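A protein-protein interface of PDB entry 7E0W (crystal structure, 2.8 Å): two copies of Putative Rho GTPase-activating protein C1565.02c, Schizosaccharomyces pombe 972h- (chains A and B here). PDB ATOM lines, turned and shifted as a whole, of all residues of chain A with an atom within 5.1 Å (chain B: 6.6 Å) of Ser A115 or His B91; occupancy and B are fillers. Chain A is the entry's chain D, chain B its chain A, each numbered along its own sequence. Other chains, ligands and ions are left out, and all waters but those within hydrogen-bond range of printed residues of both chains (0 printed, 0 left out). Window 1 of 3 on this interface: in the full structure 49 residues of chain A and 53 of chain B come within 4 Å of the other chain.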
ATOM      1  N   ARG A 111      -7.750 -11.617  32.667  1.00  0.00           N
ATOM      2  CA  ARG A 111      -7.712 -12.380  31.422  1.00  0.00           C
ATOM      3  C   ARG A 111      -8.996 -13.164  31.173  1.00  0.00           C
ATOM      4  O   ARG A 111      -9.286 -13.506  30.021  1.00  0.00           O
ATOM      5  CB  ARG A 111      -6.517 -13.334  31.431  1.00  0.00           C
ATOM      6  CG  ARG A 111      -5.792 -13.437  30.104  1.00  0.00           C
ATOM      7  CD  ARG A 111      -4.316 -13.676  30.336  1.00  0.00           C
ATOM      8  NE  ARG A 111      -4.095 -14.610  31.436  1.00  0.00           N
ATOM      9  CZ  ARG A 111      -2.981 -14.665  32.158  1.00  0.00           C
ATOM     10  NH1 ARG A 111      -1.973 -13.845  31.889  1.00  0.00           N
ATOM     11  NH2 ARG A 111      -2.867 -15.548  33.140  1.00  0.00           N
ATOM     12  N   THR A 112      -9.768 -13.455  32.224  1.00  0.00           N
ATOM     13  CA  THR A 112     -11.042 -14.142  32.043  1.00  0.00           C
ATOM     14  C   THR A 112     -12.047 -13.256  31.312  1.00  0.00           C
ATOM     15  O   THR A 112     -12.663 -13.683  30.330  1.00  0.00           O
ATOM     16  CB  THR A 112     -11.604 -14.582  33.398  1.00  0.00           C
ATOM     17  OG1 THR A 112     -10.826 -15.668  33.915  1.00  0.00           O
ATOM     18  CG2 THR A 112     -13.053 -15.032  33.257  1.00  0.00           C
ATOM     19  N   LEU A 113     -12.215 -12.009  31.768  1.00  0.00           N
ATOM     20  CA  LEU A 113     -13.272 -11.169  31.211  1.00  0.00           C
ATOM     21  C   LEU A 113     -12.943 -10.696  29.802  1.00  0.00           C
ATOM     22  O   LEU A 113     -13.857 -10.510  28.990  1.00  0.00           O
ATOM     23  CB  LEU A 113     -13.561  -9.976  32.130  1.00  0.00           C
ATOM     24  CG  LEU A 113     -12.702  -8.712  32.249  1.00  0.00           C
ATOM     25  CD1 LEU A 113     -12.866  -7.746  31.073  1.00  0.00           C
ATOM     26  CD2 LEU A 113     -13.092  -8.016  33.532  1.00  0.00           C
ATOM     27  N   LEU A 114     -11.664 -10.468  29.498  1.00  0.00           N
ATOM     28  CA  LEU A 114     -11.288 -10.195  28.116  1.00  0.00           C
ATOM     29  C   LEU A 114     -11.597 -11.389  27.228  1.00  0.00           C
ATOM     30  O   LEU A 114     -12.100 -11.230  26.109  1.00  0.00           O
ATOM     31  CB  LEU A 114      -9.803  -9.848  28.017  1.00  0.00           C
ATOM     32  CG  LEU A 114      -9.271  -8.520  28.543  1.00  0.00           C
ATOM     33  CD1 LEU A 114      -8.948  -8.614  30.005  1.00  0.00           C
ATOM     34  CD2 LEU A 114      -8.029  -8.180  27.765  1.00  0.00           C
ATOM     35  N   SER A 115     -11.294 -12.595  27.715  1.00  0.00           N
ATOM     36  CA  SER A 115     -11.592 -13.805  26.958  1.00  0.00           C
ATOM     37  C   SER A 115     -13.081 -13.902  26.652  1.00  0.00           C
ATOM     38  O   SER A 115     -13.471 -14.318  25.555  1.00  0.00           O
ATOM     39  CB  SER A 115     -11.119 -15.032  27.734  1.00  0.00           C
ATOM     40  OG  SER A 115      -9.718 -14.996  27.950  1.00  0.00           O
ATOM     41  N   ILE A 116     -13.926 -13.523  27.614  1.00  0.00           N
ATOM     42  CA  ILE A 116     -15.358 -13.416  27.347  1.00  0.00           C
ATOM     43  C   ILE A 116     -15.623 -12.305  26.340  1.00  0.00           C
ATOM     44  O   ILE A 116     -16.428 -12.463  25.412  1.00  0.00           O
ATOM     45  CB  ILE A 116     -16.133 -13.184  28.659  1.00  0.00           C
ATOM     46  CG1 ILE A 116     -15.768 -14.238  29.708  1.00  0.00           C
ATOM     47  CG2 ILE A 116     -17.631 -13.189  28.403  1.00  0.00           C
ATOM     48  CD1 ILE A 116     -16.450 -14.026  31.052  1.00  0.00           C
ATOM     49  N   ALA A 117     -14.939 -11.169  26.497  1.00  0.00           N
ATOM     50  CA  ALA A 117     -15.162 -10.032  25.609  1.00  0.00           C
ATOM     51  C   ALA A 117     -14.671 -10.326  24.197  1.00  0.00           C
ATOM     52  O   ALA A 117     -15.423 -10.174  23.228  1.00  0.00           O
ATOM     53  CB  ALA A 117     -14.472  -8.789  26.170  1.00  0.00           C
ATOM     54  N   SER A 118     -13.412 -10.748  24.061  1.00  0.00           N
ATOM     55  CA  SER A 118     -12.801 -10.993  22.759  1.00  0.00           C
ATOM     56  C   SER A 118     -13.560 -12.077  22.001  1.00  0.00           C
ATOM     57  O   SER A 118     -13.476 -13.258  22.359  1.00  0.00           O
ATOM     58  CB  SER A 118     -11.333 -11.392  22.917  1.00  0.00           C
ATOM     59  OG  SER A 118     -11.209 -12.618  23.616  1.00  0.00           O
ATOM     60  N   PHE A 121     -11.902 -15.181  19.734  1.00  0.00           N
ATOM     61  CA  PHE A 121     -11.473 -16.383  20.434  1.00  0.00           C
ATOM     62  C   PHE A 121     -12.637 -17.318  20.739  1.00  0.00           C
ATOM     63  O   PHE A 121     -12.489 -18.541  20.643  1.00  0.00           O
ATOM     64  CB  PHE A 121     -10.753 -16.000  21.730  1.00  0.00           C
ATOM     65  CG  PHE A 121     -10.714 -17.098  22.754  1.00  0.00           C
ATOM     66  CD1 PHE A 121      -9.788 -18.122  22.654  1.00  0.00           C
ATOM     67  CD2 PHE A 121     -11.594 -17.100  23.826  1.00  0.00           C
ATOM     68  CE1 PHE A 121      -9.745 -19.132  23.594  1.00  0.00           C
ATOM     69  CE2 PHE A 121     -11.556 -18.109  24.770  1.00  0.00           C
ATOM     70  CZ  PHE A 121     -10.630 -19.126  24.654  1.00  0.00           C
ATOM     71  N   THR A 122     -13.802 -16.769  21.090  1.00  0.00           N
ATOM     72  CA  THR A 122     -14.953 -17.592  21.449  1.00  0.00           C
ATOM     73  C   THR A 122     -15.587 -18.299  20.255  1.00  0.00           C
ATOM     74  O   THR A 122     -16.573 -19.021  20.448  1.00  0.00           O
ATOM     75  CB  THR A 122     -16.014 -16.744  22.161  1.00  0.00           C
ATOM     76  OG1 THR A 122     -16.836 -16.078  21.194  1.00  0.00           O
ATOM     77  CG2 THR A 122     -15.366 -15.709  23.069  1.00  0.00           C
ATOM     78  N   LYS A 124     -13.662 -20.228  17.830  1.00  0.00           N
ATOM     79  CA  LYS A 124     -12.926 -21.458  17.564  1.00  0.00           C
ATOM     80  C   LYS A 124     -13.460 -22.624  18.391  1.00  0.00           C
ATOM     81  O   LYS A 124     -12.946 -23.744  18.301  1.00  0.00           O
ATOM     82  CB  LYS A 124     -11.426 -21.249  17.839  1.00  0.00           C
ATOM     83  CG  LYS A 124     -10.982 -19.794  17.816  1.00  0.00           C
ATOM     84  CD  LYS A 124      -9.523 -19.689  17.405  1.00  0.00           C
ATOM     85  CE  LYS A 124      -8.927 -18.350  17.808  1.00  0.00           C
ATOM     86  NZ  LYS A 124      -7.435 -18.352  17.749  1.00  0.00           N
ATOM     87  N   ARG B  60       0.880 -23.237  17.080  1.00  0.00           N
ATOM     88  CA  ARG B  60      -0.502 -23.535  16.735  1.00  0.00           C
ATOM     89  C   ARG B  60      -0.875 -24.927  17.228  1.00  0.00           C
ATOM     90  O   ARG B  60      -0.071 -25.861  17.175  1.00  0.00           O
ATOM     91  CB  ARG B  60      -0.705 -23.417  15.235  1.00  0.00           C
ATOM     92  CG  ARG B  60      -0.392 -22.037  14.669  1.00  0.00           C
ATOM     93  CD  ARG B  60      -1.311 -20.955  15.253  1.00  0.00           C
ATOM     94  NE  ARG B  60      -2.666 -20.965  14.694  1.00  0.00           N
ATOM     95  CZ  ARG B  60      -3.567 -20.004  14.899  1.00  0.00           C
ATOM     96  NH1 ARG B  60      -3.255 -18.952  15.643  1.00  0.00           N
ATOM     97  NH2 ARG B  60      -4.778 -20.090  14.361  1.00  0.00           N
ATOM     98  N   TYR B  61      -2.095 -25.053  17.736  1.00  0.00           N
ATOM     99  CA  TYR B  61      -2.530 -26.301  18.345  1.00  0.00           C
ATOM    100  C   TYR B  61      -4.048 -26.332  18.374  1.00  0.00           C
ATOM    101  O   TYR B  61      -4.713 -25.303  18.223  1.00  0.00           O
ATOM    102  CB  TYR B  61      -1.957 -26.461  19.759  1.00  0.00           C
ATOM    103  CG  TYR B  61      -2.595 -25.550  20.785  1.00  0.00           C
ATOM    104  CD1 TYR B  61      -2.120 -24.262  20.989  1.00  0.00           C
ATOM    105  CD2 TYR B  61      -3.673 -25.980  21.550  1.00  0.00           C
ATOM    106  CE1 TYR B  61      -2.703 -23.425  21.924  1.00  0.00           C
ATOM    107  CE2 TYR B  61      -4.261 -25.153  22.481  1.00  0.00           C
ATOM    108  CZ  TYR B  61      -3.773 -23.877  22.666  1.00  0.00           C
ATOM    109  OH  TYR B  61      -4.357 -23.051  23.598  1.00  0.00           O
ATOM    110  N   ALA B  82     -11.559 -22.061  33.857  1.00  0.00           N
ATOM    111  CA  ALA B  82     -10.112 -22.075  34.038  1.00  0.00           C
ATOM    112  C   ALA B  82      -9.392 -21.744  32.736  1.00  0.00           C
ATOM    113  O   ALA B  82      -8.404 -21.001  32.739  1.00  0.00           O
ATOM    114  CB  ALA B  82      -9.668 -23.436  34.571  1.00  0.00           C
ATOM    115  N   TYR B  83      -9.876 -22.281  31.612  1.00  0.00           N
ATOM    116  CA  TYR B  83      -9.239 -22.016  30.325  1.00  0.00           C
ATOM    117  C   TYR B  83      -9.344 -20.544  29.951  1.00  0.00           C
ATOM    118  O   TYR B  83      -8.378 -19.952  29.457  1.00  0.00           O
ATOM    119  CB  TYR B  83      -9.868 -22.895  29.240  1.00  0.00           C
ATOM    120  CG  TYR B  83      -9.142 -22.876  27.907  1.00  0.00           C
ATOM    121  CD1 TYR B  83      -7.817 -22.471  27.820  1.00  0.00           C
ATOM    122  CD2 TYR B  83      -9.785 -23.261  26.736  1.00  0.00           C
ATOM    123  CE1 TYR B  83      -7.150 -22.449  26.607  1.00  0.00           C
ATOM    124  CE2 TYR B  83      -9.125 -23.243  25.516  1.00  0.00           C
ATOM    125  CZ  TYR B  83      -7.807 -22.836  25.459  1.00  0.00           C
ATOM    126  OH  TYR B  83      -7.138 -22.812  24.256  1.00  0.00           O
ATOM    127  N   TYR B  84     -10.506 -19.932  30.193  1.00  0.00           N
ATOM    128  CA  TYR B  84     -10.704 -18.533  29.827  1.00  0.00           C
ATOM    129  C   TYR B  84      -9.763 -17.595  30.574  1.00  0.00           C
ATOM    130  O   TYR B  84      -9.535 -16.473  30.110  1.00  0.00           O
ATOM    131  CB  TYR B  84     -12.158 -18.125  30.077  1.00  0.00           C
ATOM    132  CG  TYR B  84     -13.075 -18.397  28.905  1.00  0.00           C
ATOM    133  CD1 TYR B  84     -13.381 -19.698  28.530  1.00  0.00           C
ATOM    134  CD2 TYR B  84     -13.628 -17.356  28.170  1.00  0.00           C
ATOM    135  CE1 TYR B  84     -14.214 -19.956  27.457  1.00  0.00           C
ATOM    136  CE2 TYR B  84     -14.463 -17.604  27.095  1.00  0.00           C
ATOM    137  CZ  TYR B  84     -14.752 -18.907  26.743  1.00  0.00           C
ATOM    138  OH  TYR B  84     -15.583 -19.163  25.676  1.00  0.00           O
ATOM    139  N   GLY B  85      -9.209 -18.022  31.706  1.00  0.00           N
ATOM    140  CA  GLY B  85      -8.328 -17.168  32.480  1.00  0.00           C
ATOM    141  C   GLY B  85      -6.851 -17.445  32.293  1.00  0.00           C
ATOM    142  O   GLY B  85      -6.041 -17.151  33.179  1.00  0.00           O
ATOM    143  N   MET B  86      -6.486 -18.009  31.146  1.00  0.00           N
ATOM    144  CA  MET B  86      -5.104 -18.351  30.841  1.00  0.00           C
ATOM    145  C   MET B  86      -4.463 -17.323  29.915  1.00  0.00           C
ATOM    146  O   MET B  86      -5.145 -16.540  29.247  1.00  0.00           O
ATOM    147  CB  MET B  86      -5.011 -19.749  30.220  1.00  0.00           C
ATOM    148  CG  MET B  86      -5.243 -20.846  31.223  1.00  0.00           C
ATOM    149  SD  MET B  86      -4.093 -22.211  31.023  1.00  0.00           S
ATOM    150  CE  MET B  86      -4.922 -23.138  29.744  1.00  0.00           C
ATOM    151  N   ASP B  87      -3.125 -17.347  29.885  1.00  0.00           N
ATOM    152  CA  ASP B  87      -2.337 -16.342  29.179  1.00  0.00           C
ATOM    153  C   ASP B  87      -2.861 -16.126  27.769  1.00  0.00           C
ATOM    154  O   ASP B  87      -3.294 -17.067  27.099  1.00  0.00           O
ATOM    155  CB  ASP B  87      -0.865 -16.760  29.137  1.00  0.00           C
ATOM    156  CG  ASP B  87      -0.270 -16.906  30.519  1.00  0.00           C
ATOM    157  OD1 ASP B  87       0.496 -17.863  30.741  1.00  0.00           O
ATOM    158  OD2 ASP B  87      -0.576 -16.065  31.387  1.00  0.00           O
ATOM    159  N   TYR B  88      -2.821 -14.866  27.332  1.00  0.00           N
ATOM    160  CA  TYR B  88      -3.481 -14.479  26.089  1.00  0.00           C
ATOM    161  C   TYR B  88      -2.979 -15.299  24.906  1.00  0.00           C
ATOM    162  O   TYR B  88      -3.778 -15.729  24.066  1.00  0.00           O
ATOM    163  CB  TYR B  88      -3.278 -12.979  25.854  1.00  0.00           C
ATOM    164  CG  TYR B  88      -3.311 -12.515  24.407  1.00  0.00           C
ATOM    165  CD1 TYR B  88      -2.328 -11.667  23.920  1.00  0.00           C
ATOM    166  CD2 TYR B  88      -4.347 -12.876  23.547  1.00  0.00           C
ATOM    167  CE1 TYR B  88      -2.345 -11.227  22.609  1.00  0.00           C
ATOM    168  CE2 TYR B  88      -4.371 -12.442  22.231  1.00  0.00           C
ATOM    169  CZ  TYR B  88      -3.369 -11.615  21.769  1.00  0.00           C
ATOM    170  OH  TYR B  88      -3.391 -11.172  20.465  1.00  0.00           O
ATOM    171  N   TYR B  89      -1.666 -15.546  24.832  1.00  0.00           N
ATOM    172  CA  TYR B  89      -1.125 -16.294  23.700  1.00  0.00           C
ATOM    173  C   TYR B  89      -1.839 -17.631  23.533  1.00  0.00           C
ATOM    174  O   TYR B  89      -2.211 -18.008  22.415  1.00  0.00           O
ATOM    175  CB  TYR B  89       0.391 -16.487  23.855  1.00  0.00           C
ATOM    176  CG  TYR B  89       0.828 -17.644  24.733  1.00  0.00           C
ATOM    177  CD1 TYR B  89       1.012 -17.475  26.098  1.00  0.00           C
ATOM    178  CD2 TYR B  89       1.075 -18.902  24.191  1.00  0.00           C
ATOM    179  CE1 TYR B  89       1.418 -18.525  26.900  1.00  0.00           C
ATOM    180  CE2 TYR B  89       1.481 -19.956  24.983  1.00  0.00           C
ATOM    181  CZ  TYR B  89       1.651 -19.762  26.336  1.00  0.00           C
ATOM    182  OH  TYR B  89       2.053 -20.811  27.129  1.00  0.00           O
ATOM    183  N   LEU B  90      -2.088 -18.334  24.640  1.00  0.00           N
ATOM    184  CA  LEU B  90      -2.815 -19.598  24.581  1.00  0.00           C
ATOM    185  C   LEU B  90      -4.200 -19.450  23.966  1.00  0.00           C
ATOM    186  O   LEU B  90      -4.780 -20.451  23.536  1.00  0.00           O
ATOM    187  CB  LEU B  90      -2.934 -20.200  25.980  1.00  0.00           C
ATOM    188  CG  LEU B  90      -1.644 -20.781  26.550  1.00  0.00           C
ATOM    189  CD1 LEU B  90      -1.786 -21.021  28.042  1.00  0.00           C
ATOM    190  CD2 LEU B  90      -1.276 -22.065  25.823  1.00  0.00           C
ATOM    191  N   HIS B  91      -4.745 -18.233  23.919  1.00  0.00           N
ATOM    192  CA  HIS B  91      -6.016 -17.997  23.247  1.00  0.00           C
ATOM    193  C   HIS B  91      -5.856 -17.713  21.760  1.00  0.00           C
ATOM    194  O   HIS B  91      -6.738 -18.083  20.975  1.00  0.00           O
ATOM    195  CB  HIS B  91      -6.760 -16.831  23.908  1.00  0.00           C
ATOM    196  CG  HIS B  91      -7.198 -17.112  25.311  1.00  0.00           C
ATOM    197  ND1 HIS B  91      -7.420 -18.390  25.775  1.00  0.00           N
ATOM    198  CD2 HIS B  91      -7.459 -16.283  26.350  1.00  0.00           C
ATOM    199  CE1 HIS B  91      -7.798 -18.338  27.039  1.00  0.00           C
ATOM    200  NE2 HIS B  91      -7.830 -17.071  27.413  1.00  0.00           N
ATOM    201  N   LYS B  92      -4.756 -17.069  21.344  1.00  0.00           N
ATOM    202  CA  LYS B  92      -4.593 -16.738  19.933  1.00  0.00           C
ATOM    203  C   LYS B  92      -4.179 -17.972  19.131  1.00  0.00           C
ATOM    204  O   LYS B  92      -4.812 -18.282  18.117  1.00  0.00           O
ATOM    205  CB  LYS B  92      -3.594 -15.567  19.786  1.00  0.00           C
ATOM    206  CG  LYS B  92      -3.000 -15.200  18.373  1.00  0.00           C
ATOM    207  CD  LYS B  92      -3.902 -15.500  17.147  1.00  0.00           C
ATOM    208  CE  LYS B  92      -5.299 -14.897  17.192  1.00  0.00           C
ATOM    209  NZ  LYS B  92      -6.124 -15.618  16.193  1.00  0.00           N
ATOM    210  N   ASN B  93      -3.234 -18.765  19.638  1.00  0.00           N
ATOM    211  CA  ASN B  93      -2.638 -19.847  18.863  1.00  0.00           C
ATOM    212  C   ASN B  93      -3.544 -21.075  18.719  1.00  0.00           C
ATOM    213  O   ASN B  93      -3.092 -22.099  18.193  1.00  0.00           O
ATOM    214  CB  ASN B  93      -1.303 -20.259  19.489  1.00  0.00           C
ATOM    215  CG  ASN B  93      -0.419 -19.067  19.857  1.00  0.00           C
ATOM    216  OD1 ASN B  93      -0.097 -18.850  21.029  1.00  0.00           O
ATOM    217  ND2 ASN B  93      -0.023 -18.294  18.853  1.00  0.00           N
ATOM    218  N   VAL B  94      -4.801 -20.999  19.154  1.00  0.00           N
ATOM    219  CA  VAL B  94      -5.718 -22.123  19.004  1.00  0.00           C
ATOM    220  C   VAL B  94      -6.177 -22.216  17.558  1.00  0.00           C
ATOM    221  O   VAL B  94      -6.612 -21.221  16.963  1.00  0.00           O
ATOM    222  CB  VAL B  94      -6.929 -21.980  19.937  1.00  0.00           C
ATOM    223  CG1 VAL B  94      -7.559 -23.343  20.159  1.00  0.00           C
ATOM    224  CG2 VAL B  94      -6.541 -21.346  21.247  1.00  0.00           C
ATOM    225  N   ARG B 111     -22.269 -18.009  29.718  1.00  0.00           N
ATOM    226  CA  ARG B 111     -21.086 -17.425  29.091  1.00  0.00           C
ATOM    227  C   ARG B 111     -21.447 -16.740  27.779  1.00  0.00           C
ATOM    228  O   ARG B 111     -21.010 -15.613  27.514  1.00  0.00           O
ATOM    229  CB  ARG B 111     -20.021 -18.503  28.861  1.00  0.00           C
ATOM    230  CG  ARG B 111     -18.596 -17.977  28.635  1.00  0.00           C
ATOM    231  CD  ARG B 111     -18.360 -17.510  27.196  1.00  0.00           C
ATOM    232  NE  ARG B 111     -18.744 -18.522  26.216  1.00  0.00           N
ATOM    233  CZ  ARG B 111     -19.009 -18.264  24.938  1.00  0.00           C
ATOM    234  NH1 ARG B 111     -18.938 -17.022  24.479  1.00  0.00           N
ATOM    235  NH2 ARG B 111     -19.351 -19.250  24.120  1.00  0.00           N
ATOM    236  N   SER B 115     -20.749 -12.751  26.836  1.00  0.00           N
ATOM    237  CA  SER B 115     -20.054 -12.249  25.656  1.00  0.00           C
ATOM    238  C   SER B 115     -20.938 -11.295  24.861  1.00  0.00           C
ATOM    239  O   SER B 115     -20.448 -10.310  24.297  1.00  0.00           O
ATOM    240  CB  SER B 115     -19.599 -13.417  24.780  1.00  0.00           C
ATOM    241  OG  SER B 115     -18.712 -14.271  25.481  1.00  0.00           O
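O of Tyr B84 lies within hydrogen-bond range of OG of Ser A115 (2.6 Å). The backbone carbonyl oxygen (O) of Met B86 lies within hydrogen-bond range of the guanidinium group (NE) of Arg A111, 3.1 Å away. The guanidinium group (NH1) of Arg A111 is in salt-bridge range of the side-chain carboxylate (OD2) of Asp B87. A ring nitrogen (NE2) of His B91 lies within hydrogen-bond range of the side-chain hydroxyl (OG) of Ser A115 (2.9 Å). NZ of Lys A124 is in hydrogen-bond range of O of His B91, 3.3 Å away. NZ of Lys A124 lies within hydrogen-bond range of O of Lys B92. The backbone carbonyl oxygen (O) of Val B94 sits at hydrogen-bond distance from the side-chain amino group (NZ) of Lys A124 (3.1 Å). OG of Ser B115 is in hydrogen-bond range of O of Ile A116, 2.9 Å away. O of Arg A111 sits close to O of Tyr B84 (3.0 Å).
The guanidinium group (NH1) of Arg B60 is in hydrogen-bond range of the backbone carbonyl oxygen (O) of Lys B92, 3.0 Å away. O of Tyr B84 lies within hydrogen-bond range of NE2 of His B91 (3.2 Å). The guanidinium group of Arg B111 is in hydrogen-bond range of the side-chain hydroxyl of Tyr B84 (3.3 Å). The backbone carbonyl oxygen of Met B86 is in hydrogen-bond range of a ring nitrogen (NE2) of His B91, 3.3 Å away. The side-chain hydroxyl (OG) of Ser B115 lies within hydrogen-bond range of the guanidinium group (NH1) of Arg B111. The backbone carbonyl oxygen of Arg A111 lies within hydrogen-bond range of the side-chain hydroxyl of Ser A115, 2.6 Å away.
Gly B85 touches Arg A111 (O to NH2, 3.6 Å). Arg A111 touches Tyr B88. Tyr B84 touches Thr A112. Gly B85 touches Thr A112 (CA to OG1, 3.2 Å). Ile A116 touches Tyr B84 (N to CD2, 3.9 Å). Tyr B84 touches Phe A121. His B91 touches Phe A121 (ND1 to CE1, 3.3 Å). Thr A122 touches Arg B111 (CB to NH1, 3.7 Å).
Ser A115 touches two residues of chain B. Of the printed residues of chain A, Arg B111 touches Thr A122. Printed residues of chain A within 4 Å of Asp B87: Arg A111. Of the printed residues of chain A, Val B94 touches Lys A124 (3.1 Å). Of the printed residues of chain B, Arg A111 touches Tyr B84 (3.0 Å), Gly B85 (3.6 Å), Met B86 (3.1 Å), Asp B87 (2.7 Å) and Tyr B88 (3.6 Å). Leu B90 touches none of the printed residues of chain A. Ser A118 touches none of the printed residues of chain B. The nearest printed residue of chain B that does not touch Thr A122 is Tyr B84 (4.3 Å).
Hydrophobic or aromatic side chains of chain A within 4 Å of the printed part of chain B: Ile A116 and Phe A121. Of the 17 printed residues of chain B, 10 touch a printed residue of chain A. Printed residues of chain B that touch a printed residue of chain A: Tyr B84, Gly B85, Met B86, Asp B87, Tyr B88, His B91, Lys B92, Val B94, Arg B111 and Ser B115. Hydrophobic or aromatic side chains of chain B within 4 Å of the printed part of chain A: Tyr B84 and His B91. Among the printed residues, Asp or Glu carboxylates within 4 Å of a Lys or Arg side-chain nitrogen of the other chain: Arg A111 with Asp B87 (2.7 Å).
2 positions are printed for both chains.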
